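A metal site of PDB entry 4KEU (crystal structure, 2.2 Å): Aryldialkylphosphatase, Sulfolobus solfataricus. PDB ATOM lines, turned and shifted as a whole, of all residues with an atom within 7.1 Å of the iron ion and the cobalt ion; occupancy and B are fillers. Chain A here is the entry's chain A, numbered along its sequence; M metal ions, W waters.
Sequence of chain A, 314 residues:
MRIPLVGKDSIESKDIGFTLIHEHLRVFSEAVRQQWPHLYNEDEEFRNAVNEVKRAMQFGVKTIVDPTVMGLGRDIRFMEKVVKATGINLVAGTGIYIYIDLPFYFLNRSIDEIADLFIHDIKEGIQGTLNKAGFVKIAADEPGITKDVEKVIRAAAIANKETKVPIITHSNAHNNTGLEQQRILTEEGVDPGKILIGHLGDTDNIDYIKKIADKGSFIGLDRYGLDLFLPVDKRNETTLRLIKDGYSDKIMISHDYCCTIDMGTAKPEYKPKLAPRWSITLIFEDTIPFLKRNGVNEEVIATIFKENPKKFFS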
ATOM      1  N   HIS A  22     -10.385  14.162   9.281  1.00  0.00           N
ATOM      2  CA  HIS A  22     -10.296  14.855   7.999  1.00  0.00           C
ATOM      3  C   HIS A  22     -10.298  16.368   8.170  1.00  0.00           C
ATOM      4  O   HIS A  22     -11.397  17.035   8.176  1.00  0.00           O
ATOM      5  CB  HIS A  22     -11.473  14.404   7.028  1.00  0.00           C
ATOM      6  CG  HIS A  22     -11.295  14.898   5.536  1.00  0.00           C
ATOM      7  ND1 HIS A  22     -11.488  14.063   4.443  1.00  0.00           N
ATOM      8  CD2 HIS A  22     -10.935  16.156   5.008  1.00  0.00           C
ATOM      9  CE1 HIS A  22     -11.275  14.756   3.289  1.00  0.00           C
ATOM     10  NE2 HIS A  22     -10.927  16.030   3.619  1.00  0.00           N
ATOM     11  N   GLU A  23      -9.093  16.936   8.308  1.00  0.00           N
ATOM     12  CA  GLU A  23      -8.929  18.386   8.365  1.00  0.00           C
ATOM     13  C   GLU A  23      -7.708  18.781   7.563  1.00  0.00           C
ATOM     14  O   GLU A  23      -6.780  18.011   7.429  1.00  0.00           O
ATOM     15  CB  GLU A  23      -8.771  18.892   9.844  1.00  0.00           C
ATOM     16  CG  GLU A  23      -9.797  18.320  10.850  1.00  0.00           C
ATOM     17  CD  GLU A  23     -11.220  18.843  10.630  1.00  0.00           C
ATOM     18  OE1 GLU A  23     -12.187  18.155  11.100  1.00  0.00           O
ATOM     19  OE2 GLU A  23     -11.390  19.966   9.983  1.00  0.00           O
ATOM     20  N   HIS A  24      -7.717  20.018   7.027  1.00  0.00           N
ATOM     21  CA  HIS A  24      -6.557  20.534   6.254  1.00  0.00           C
ATOM     22  C   HIS A  24      -5.913  21.730   6.941  1.00  0.00           C
ATOM     23  O   HIS A  24      -6.570  22.708   7.231  1.00  0.00           O
ATOM     24  CB  HIS A  24      -6.985  20.930   4.841  1.00  0.00           C
ATOM     25  CG  HIS A  24      -7.702  19.821   4.076  1.00  0.00           C
ATOM     26  ND1 HIS A  24      -7.035  18.897   3.314  1.00  0.00           N
ATOM     27  CD2 HIS A  24      -9.068  19.509   3.946  1.00  0.00           C
ATOM     28  CE1 HIS A  24      -7.929  18.043   2.748  1.00  0.00           C
ATOM     29  NE2 HIS A  24      -9.154  18.409   3.121  1.00  0.00           N
ATOM     30  N   VAL A  27      -4.496  24.374   2.074  1.00  0.00           N
ATOM     31  CA  VAL A  27      -4.713  23.842   0.748  1.00  0.00           C
ATOM     32  C   VAL A  27      -4.418  24.892  -0.332  1.00  0.00           C
ATOM     33  O   VAL A  27      -4.798  26.040  -0.199  1.00  0.00           O
ATOM     34  CB  VAL A  27      -6.175  23.319   0.564  1.00  0.00           C
ATOM     35  CG1 VAL A  27      -6.439  23.006  -0.886  1.00  0.00           C
ATOM     36  CG2 VAL A  27      -6.419  22.102   1.417  1.00  0.00           C
ATOM     37  N   PRO A  67      -5.584  14.973   5.055  1.00  0.00           N
ATOM     38  CA  PRO A  67      -5.514  14.341   3.705  1.00  0.00           C
ATOM     39  C   PRO A  67      -5.132  15.303   2.560  1.00  0.00           C
ATOM     40  O   PRO A  67      -5.630  15.154   1.433  1.00  0.00           O
ATOM     41  CB  PRO A  67      -6.924  13.800   3.502  1.00  0.00           C
ATOM     42  CG  PRO A  67      -7.808  14.739   4.276  1.00  0.00           C
ATOM     43  CD  PRO A  67      -6.970  15.307   5.429  1.00  0.00           C
ATOM     44  N   THR A  68      -4.273  16.268   2.842  1.00  0.00           N
ATOM     45  CA  THR A  68      -3.718  17.121   1.804  1.00  0.00           C
ATOM     46  C   THR A  68      -2.676  16.364   1.033  1.00  0.00           C
ATOM     47  O   THR A  68      -1.684  15.899   1.605  1.00  0.00           O
ATOM     48  CB  THR A  68      -3.052  18.432   2.413  1.00  0.00           C
ATOM     49  OG1 THR A  68      -3.911  19.008   3.378  1.00  0.00           O
ATOM     50  CG2 THR A  68      -2.782  19.434   1.351  1.00  0.00           C
ATOM     51  N   LEU A  72      -3.556  19.230  -3.823  1.00  0.00           N
ATOM     52  CA  LEU A  72      -4.071  20.073  -2.747  1.00  0.00           C
ATOM     53  C   LEU A  72      -2.953  20.875  -2.059  1.00  0.00           C
ATOM     54  O   LEU A  72      -3.204  21.609  -1.089  1.00  0.00           O
ATOM     55  CB  LEU A  72      -4.845  19.211  -1.694  1.00  0.00           C
ATOM     56  CG  LEU A  72      -6.137  18.484  -2.219  1.00  0.00           C
ATOM     57  CD1 LEU A  72      -6.703  17.565  -1.183  1.00  0.00           C
ATOM     58  CD2 LEU A  72      -7.209  19.516  -2.710  1.00  0.00           C
ATOM     59  N   TYR A  97      -5.005  13.738  -5.883  1.00  0.00           N
ATOM     60  CA  TYR A  97      -6.298  14.309  -5.843  1.00  0.00           C
ATOM     61  C   TYR A  97      -6.624  14.933  -7.193  1.00  0.00           C
ATOM     62  O   TYR A  97      -6.115  16.019  -7.524  1.00  0.00           O
ATOM     63  CB  TYR A  97      -6.352  15.367  -4.738  1.00  0.00           C
ATOM     64  CG  TYR A  97      -7.721  15.996  -4.495  1.00  0.00           C
ATOM     65  CD1 TYR A  97      -8.213  16.983  -5.339  1.00  0.00           C
ATOM     66  CD2 TYR A  97      -8.510  15.597  -3.381  1.00  0.00           C
ATOM     67  CE1 TYR A  97      -9.448  17.558  -5.117  1.00  0.00           C
ATOM     68  CE2 TYR A  97      -9.730  16.163  -3.150  1.00  0.00           C
ATOM     69  CZ  TYR A  97     -10.213  17.146  -4.014  1.00  0.00           C
ATOM     70  OH  TYR A  97     -11.422  17.716  -3.775  1.00  0.00           O
ATOM     71  N   TYR A  99     -10.026  15.113 -10.457  1.00  0.00           N
ATOM     72  CA  TYR A  99     -11.435  14.847 -10.808  1.00  0.00           C
ATOM     73  C   TYR A  99     -11.569  14.250 -12.194  1.00  0.00           C
ATOM     74  O   TYR A  99     -12.478  13.493 -12.464  1.00  0.00           O
ATOM     75  CB  TYR A  99     -12.285  16.125 -10.710  1.00  0.00           C
ATOM     76  CG  TYR A  99     -12.461  16.716  -9.284  1.00  0.00           C
ATOM     77  CD1 TYR A  99     -12.051  15.998  -8.141  1.00  0.00           C
ATOM     78  CD2 TYR A  99     -13.055  17.993  -9.090  1.00  0.00           C
ATOM     79  CE1 TYR A  99     -12.212  16.535  -6.846  1.00  0.00           C
ATOM     80  CE2 TYR A  99     -13.228  18.534  -7.816  1.00  0.00           C
ATOM     81  CZ  TYR A  99     -12.809  17.827  -6.701  1.00  0.00           C
ATOM     82  OH  TYR A  99     -12.987  18.366  -5.444  1.00  0.00           O
ATOM     83  N   KCX A 137      -4.824   8.888  -0.041  1.00  0.00           N
ATOM     84  CA  KCX A 137      -5.997   9.674  -0.334  1.00  0.00           C
ATOM     85  CB  KCX A 137      -5.757  11.125   0.172  1.00  0.00           C
ATOM     86  CG  KCX A 137      -6.810  12.127  -0.339  1.00  0.00           C
ATOM     87  CD  KCX A 137      -8.129  11.967   0.384  1.00  0.00           C
ATOM     88  CE  KCX A 137      -9.178  13.024  -0.121  1.00  0.00           C
ATOM     89  NZ  KCX A 137      -8.865  14.412   0.394  1.00  0.00           N
ATOM     90  C   KCX A 137      -6.272   9.638  -1.838  1.00  0.00           C
ATOM     91  O   KCX A 137      -5.365   9.768  -2.639  1.00  0.00           O
ATOM     92  CX  KCX A 137      -9.847  15.366   0.543  1.00  0.00           C
ATOM     93  OQ1 KCX A 137      -9.487  16.560   0.998  1.00  0.00           O
ATOM     94  OQ2 KCX A 137     -11.114  15.138   0.281  1.00  0.00           O
ATOM     95  N   ILE A 138      -7.537   9.450  -2.201  1.00  0.00           N
ATOM     96  CA  ILE A 138      -7.965   9.460  -3.612  1.00  0.00           C
ATOM     97  C   ILE A 138      -9.252  10.177  -3.702  1.00  0.00           C
ATOM     98  O   ILE A 138      -9.936  10.373  -2.695  1.00  0.00           O
ATOM     99  CB  ILE A 138      -8.176   8.036  -4.165  1.00  0.00           C
ATOM    100  CG1 ILE A 138      -9.324   7.351  -3.433  1.00  0.00           C
ATOM    101  CG2 ILE A 138      -6.864   7.221  -4.059  1.00  0.00           C
ATOM    102  CD1 ILE A 138      -9.462   5.899  -3.750  1.00  0.00           C
ATOM    103  N   ALA A 139      -9.643  10.571  -4.950  1.00  0.00           N
ATOM    104  CA  ALA A 139     -10.847  11.390  -5.129  1.00  0.00           C
ATOM    105  C   ALA A 139     -11.620  11.091  -6.411  1.00  0.00           C
ATOM    106  O   ALA A 139     -11.089  10.525  -7.356  1.00  0.00           O
ATOM    107  CB  ALA A 139     -10.478  12.903  -5.070  1.00  0.00           C
ATOM    108  N   ASP A 141     -15.304  13.132  -8.223  1.00  0.00           N
ATOM    109  CA  ASP A 141     -16.378  14.042  -8.001  1.00  0.00           C
ATOM    110  C   ASP A 141     -17.408  14.006  -9.140  1.00  0.00           C
ATOM    111  O   ASP A 141     -17.706  12.920  -9.683  1.00  0.00           O
ATOM    112  CB  ASP A 141     -15.832  15.492  -7.769  1.00  0.00           C
ATOM    113  CG  ASP A 141     -16.768  16.342  -6.881  1.00  0.00           C
ATOM    114  OD1 ASP A 141     -17.806  16.804  -7.373  1.00  0.00           O
ATOM    115  OD2 ASP A 141     -16.436  16.563  -5.701  1.00  0.00           O
ATOM    116  N   THR A 169     -11.057   8.590   1.050  1.00  0.00           N
ATOM    117  CA  THR A 169     -11.489   9.081  -0.250  1.00  0.00           C
ATOM    118  C   THR A 169     -12.231  10.371  -0.172  1.00  0.00           C
ATOM    119  O   THR A 169     -12.740  10.740   0.847  1.00  0.00           O
ATOM    120  CB  THR A 169     -12.393   8.022  -1.022  1.00  0.00           C
ATOM    121  OG1 THR A 169     -13.758   8.151  -0.604  1.00  0.00           O
ATOM    122  CG2 THR A 169     -11.910   6.621  -0.774  1.00  0.00           C
ATOM    123  N   HIS A 170     -12.258  11.055  -1.275  1.00  0.00           N
ATOM    124  CA  HIS A 170     -13.088  12.147  -1.484  1.00  0.00           C
ATOM    125  C   HIS A 170     -14.090  11.711  -2.477  1.00  0.00           C
ATOM    126  O   HIS A 170     -13.747  11.081  -3.477  1.00  0.00           O
ATOM    127  CB  HIS A 170     -12.251  13.332  -2.069  1.00  0.00           C
ATOM    128  CG  HIS A 170     -13.091  14.476  -2.600  1.00  0.00           C
ATOM    129  ND1 HIS A 170     -13.135  15.718  -1.993  1.00  0.00           N
ATOM    130  CD2 HIS A 170     -13.951  14.559  -3.732  1.00  0.00           C
ATOM    131  CE1 HIS A 170     -13.960  16.537  -2.695  1.00  0.00           C
ATOM    132  NE2 HIS A 170     -14.464  15.832  -3.760  1.00  0.00           N
ATOM    133  N   SER A 171     -15.348  12.004  -2.238  1.00  0.00           N
ATOM    134  CA  SER A 171     -16.408  11.637  -3.215  1.00  0.00           C
ATOM    135  C   SER A 171     -17.506  12.685  -3.313  1.00  0.00           C
ATOM    136  O   SER A 171     -17.578  13.604  -2.515  1.00  0.00           O
ATOM    137  CB  SER A 171     -17.001  10.253  -2.891  1.00  0.00           C
ATOM    138  OG  SER A 171     -17.918  10.344  -1.855  1.00  0.00           O
ATOM    139  N   GLY A 198     -15.620   9.303   1.730  1.00  0.00           N
ATOM    140  CA  GLY A 198     -15.742  10.668   2.215  1.00  0.00           C
ATOM    141  C   GLY A 198     -16.912  11.488   1.719  1.00  0.00           C
ATOM    142  O   GLY A 198     -17.481  11.227   0.646  1.00  0.00           O
ATOM    143  N   HIS A 199     -17.268  12.487   2.511  1.00  0.00           N
ATOM    144  CA  HIS A 199     -18.251  13.499   2.143  1.00  0.00           C
ATOM    145  C   HIS A 199     -19.641  12.966   1.958  1.00  0.00           C
ATOM    146  O   HIS A 199     -20.484  13.603   1.303  1.00  0.00           O
ATOM    147  CB  HIS A 199     -17.778  14.285   0.899  1.00  0.00           C
ATOM    148  CG  HIS A 199     -16.328  14.782   1.004  1.00  0.00           C
ATOM    149  ND1 HIS A 199     -15.738  15.102   2.222  1.00  0.00           N
ATOM    150  CD2 HIS A 199     -15.369  15.011   0.027  1.00  0.00           C
ATOM    151  CE1 HIS A 199     -14.448  15.510   2.007  1.00  0.00           C
ATOM    152  NE2 HIS A 199     -14.203  15.452   0.683  1.00  0.00           N
ATOM    153  N   ASP A 222     -18.151  14.308   7.208  1.00  0.00           N
ATOM    154  CA  ASP A 222     -16.899  14.962   7.468  1.00  0.00           C
ATOM    155  C   ASP A 222     -16.797  16.394   6.942  1.00  0.00           C
ATOM    156  O   ASP A 222     -15.681  16.938   6.818  1.00  0.00           O
ATOM    157  CB  ASP A 222     -15.765  14.109   6.850  1.00  0.00           C
ATOM    158  CG  ASP A 222     -16.023  13.792   5.315  1.00  0.00           C
ATOM    159  OD1 ASP A 222     -15.432  12.820   4.802  1.00  0.00           O
ATOM    160  OD2 ASP A 222     -16.843  14.544   4.672  1.00  0.00           O
ATOM    161  N   ARG A 223     -17.913  16.998   6.651  1.00  0.00           N
ATOM    162  CA  ARG A 223     -17.894  18.412   6.187  1.00  0.00           C
ATOM    163  C   ARG A 223     -18.784  19.325   7.037  1.00  0.00           C
ATOM    164  O   ARG A 223     -19.423  20.282   6.521  1.00  0.00           O
ATOM    165  CB  ARG A 223     -18.255  18.501   4.695  1.00  0.00           C
ATOM    166  CG  ARG A 223     -17.050  18.233   3.739  1.00  0.00           C
ATOM    167  CD  ARG A 223     -17.485  18.119   2.300  1.00  0.00           C
ATOM    168  NE  ARG A 223     -16.398  18.456   1.397  1.00  0.00           N
ATOM    169  CZ  ARG A 223     -16.482  18.386   0.047  1.00  0.00           C
ATOM    170  NH1 ARG A 223     -17.605  17.967  -0.521  1.00  0.00           N
ATOM    171  NH2 ARG A 223     -15.431  18.715  -0.707  1.00  0.00           N
ATOM    172  N   ASP A 256     -13.483  18.967   7.554  1.00  0.00           N
ATOM    173  CA  ASP A 256     -12.827  19.218   6.263  1.00  0.00           C
ATOM    174  C   ASP A 256     -12.444  20.662   6.222  1.00  0.00           C
ATOM    175  O   ASP A 256     -12.505  21.309   5.187  1.00  0.00           O
ATOM    176  CB  ASP A 256     -13.787  18.891   5.103  1.00  0.00           C
ATOM    177  CG  ASP A 256     -13.054  18.765   3.683  1.00  0.00           C
ATOM    178  OD1 ASP A 256     -11.740  18.528   3.640  1.00  0.00           O
ATOM    179  OD2 ASP A 256     -13.748  18.872   2.652  1.00  0.00           O
ATOM    180  N   TYR A 257     -12.045  21.182   7.348  1.00  0.00           N
ATOM    181  CA  TYR A 257     -11.772  22.582   7.457  1.00  0.00           C
ATOM    182  C   TYR A 257     -10.405  22.948   6.918  1.00  0.00           C
ATOM    183  O   TYR A 257      -9.423  22.217   7.126  1.00  0.00           O
ATOM    184  CB  TYR A 257     -11.930  23.058   8.915  1.00  0.00           C
ATOM    185  CG  TYR A 257     -11.761  24.501   9.050  1.00  0.00           C
ATOM    186  CD1 TYR A 257     -10.579  25.042   9.594  1.00  0.00           C
ATOM    187  CD2 TYR A 257     -12.770  25.390   8.640  1.00  0.00           C
ATOM    188  CE1 TYR A 257     -10.408  26.417   9.723  1.00  0.00           C
ATOM    189  CE2 TYR A 257     -12.615  26.775   8.760  1.00  0.00           C
ATOM    190  CZ  TYR A 257     -11.438  27.283   9.304  1.00  0.00           C
ATOM    191  OH  TYR A 257     -11.275  28.632   9.420  1.00  0.00           O
ATOM    192  N   CYS A 258     -10.349  24.068   6.230  1.00  0.00           N
ATOM    193  CA  CYS A 258      -9.113  24.565   5.697  1.00  0.00           C
ATOM    194  C   CYS A 258      -8.707  25.797   6.412  1.00  0.00           C
ATOM    195  O   CYS A 258      -9.230  26.871   6.142  1.00  0.00           O
ATOM    196  CB  CYS A 258      -9.272  24.868   4.211  1.00  0.00           C
ATOM    197  SG  CYS A 258      -9.995  23.554   3.280  1.00  0.00           S
HETATM  198 FE    FE M   1     -10.646  17.502   2.296  1.00  0.00          FE
HETATM  199 CO    CO M   2     -12.636  16.141  -0.150  1.00  0.00          CO
HETATM  200  O   HOH W   1     -12.302  17.627   1.157  1.00  0.00           O
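The iron ion is bound by a ring nitrogen (NE2) of His 24, OQ1 of KCX 137, a ring nitrogen (NE2) of His 22, water W1 and the side-chain carboxylate (OD1) of Asp 256. The iron ion has five donor atoms within binding distance.
The cobalt ion is bound by OQ2 of KCX 137 (1.9 Å), NE2 of His 199 (1.9 Å), ND1 of His 170 (2.0 Å) and water W1 (2.0 Å).
A ring nitrogen (ND1) of His 199 is in hydrogen-bond range of the side-chain carboxylate (OD2) of Asp 222, at 2.7 Å. The backbone carbonyl oxygen (O) of Tyr 257 sits at hydrogen-bond distance from the backbone NH (N) of His 24. OG1 of Thr 68 is in hydrogen-bond range of ND1 of His 24. OH of Tyr 99 lies within hydrogen-bond range of NE2 of His 170, at 3.4 Å. O of Ile 138 lies within hydrogen-bond range of N of His 170 (2.8 Å). The guanidinium group of Arg 223 is in salt-bridge range of the side-chain carboxylate of Asp 256. The backbone NH (N) of Asp 256 lies within hydrogen-bond range of the side-chain carboxylate (OE2) of Glu 23, at 3.4 Å. The backbone NH of Asp 256 sits at hydrogen-bond distance from the backbone carbonyl oxygen of Asp 222, 3.1 Å away.
Arg 223 touches the cobalt ion (NH2 to CO, 3.8 Å). Five residues have an atom within 4 Å of the cobalt ion: His 22, KCX 137, His 170, His 199 and Arg 223. The nearest printed residue that does not touch the cobalt ion is Asp 256 (4.1 Å).
Four residues have an atom within 4 Å of the iron ion: His 22, His 24, KCX 137 and Asp 256. The nearest printed residue that does not touch the iron ion is His 199 (4.3 Å).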
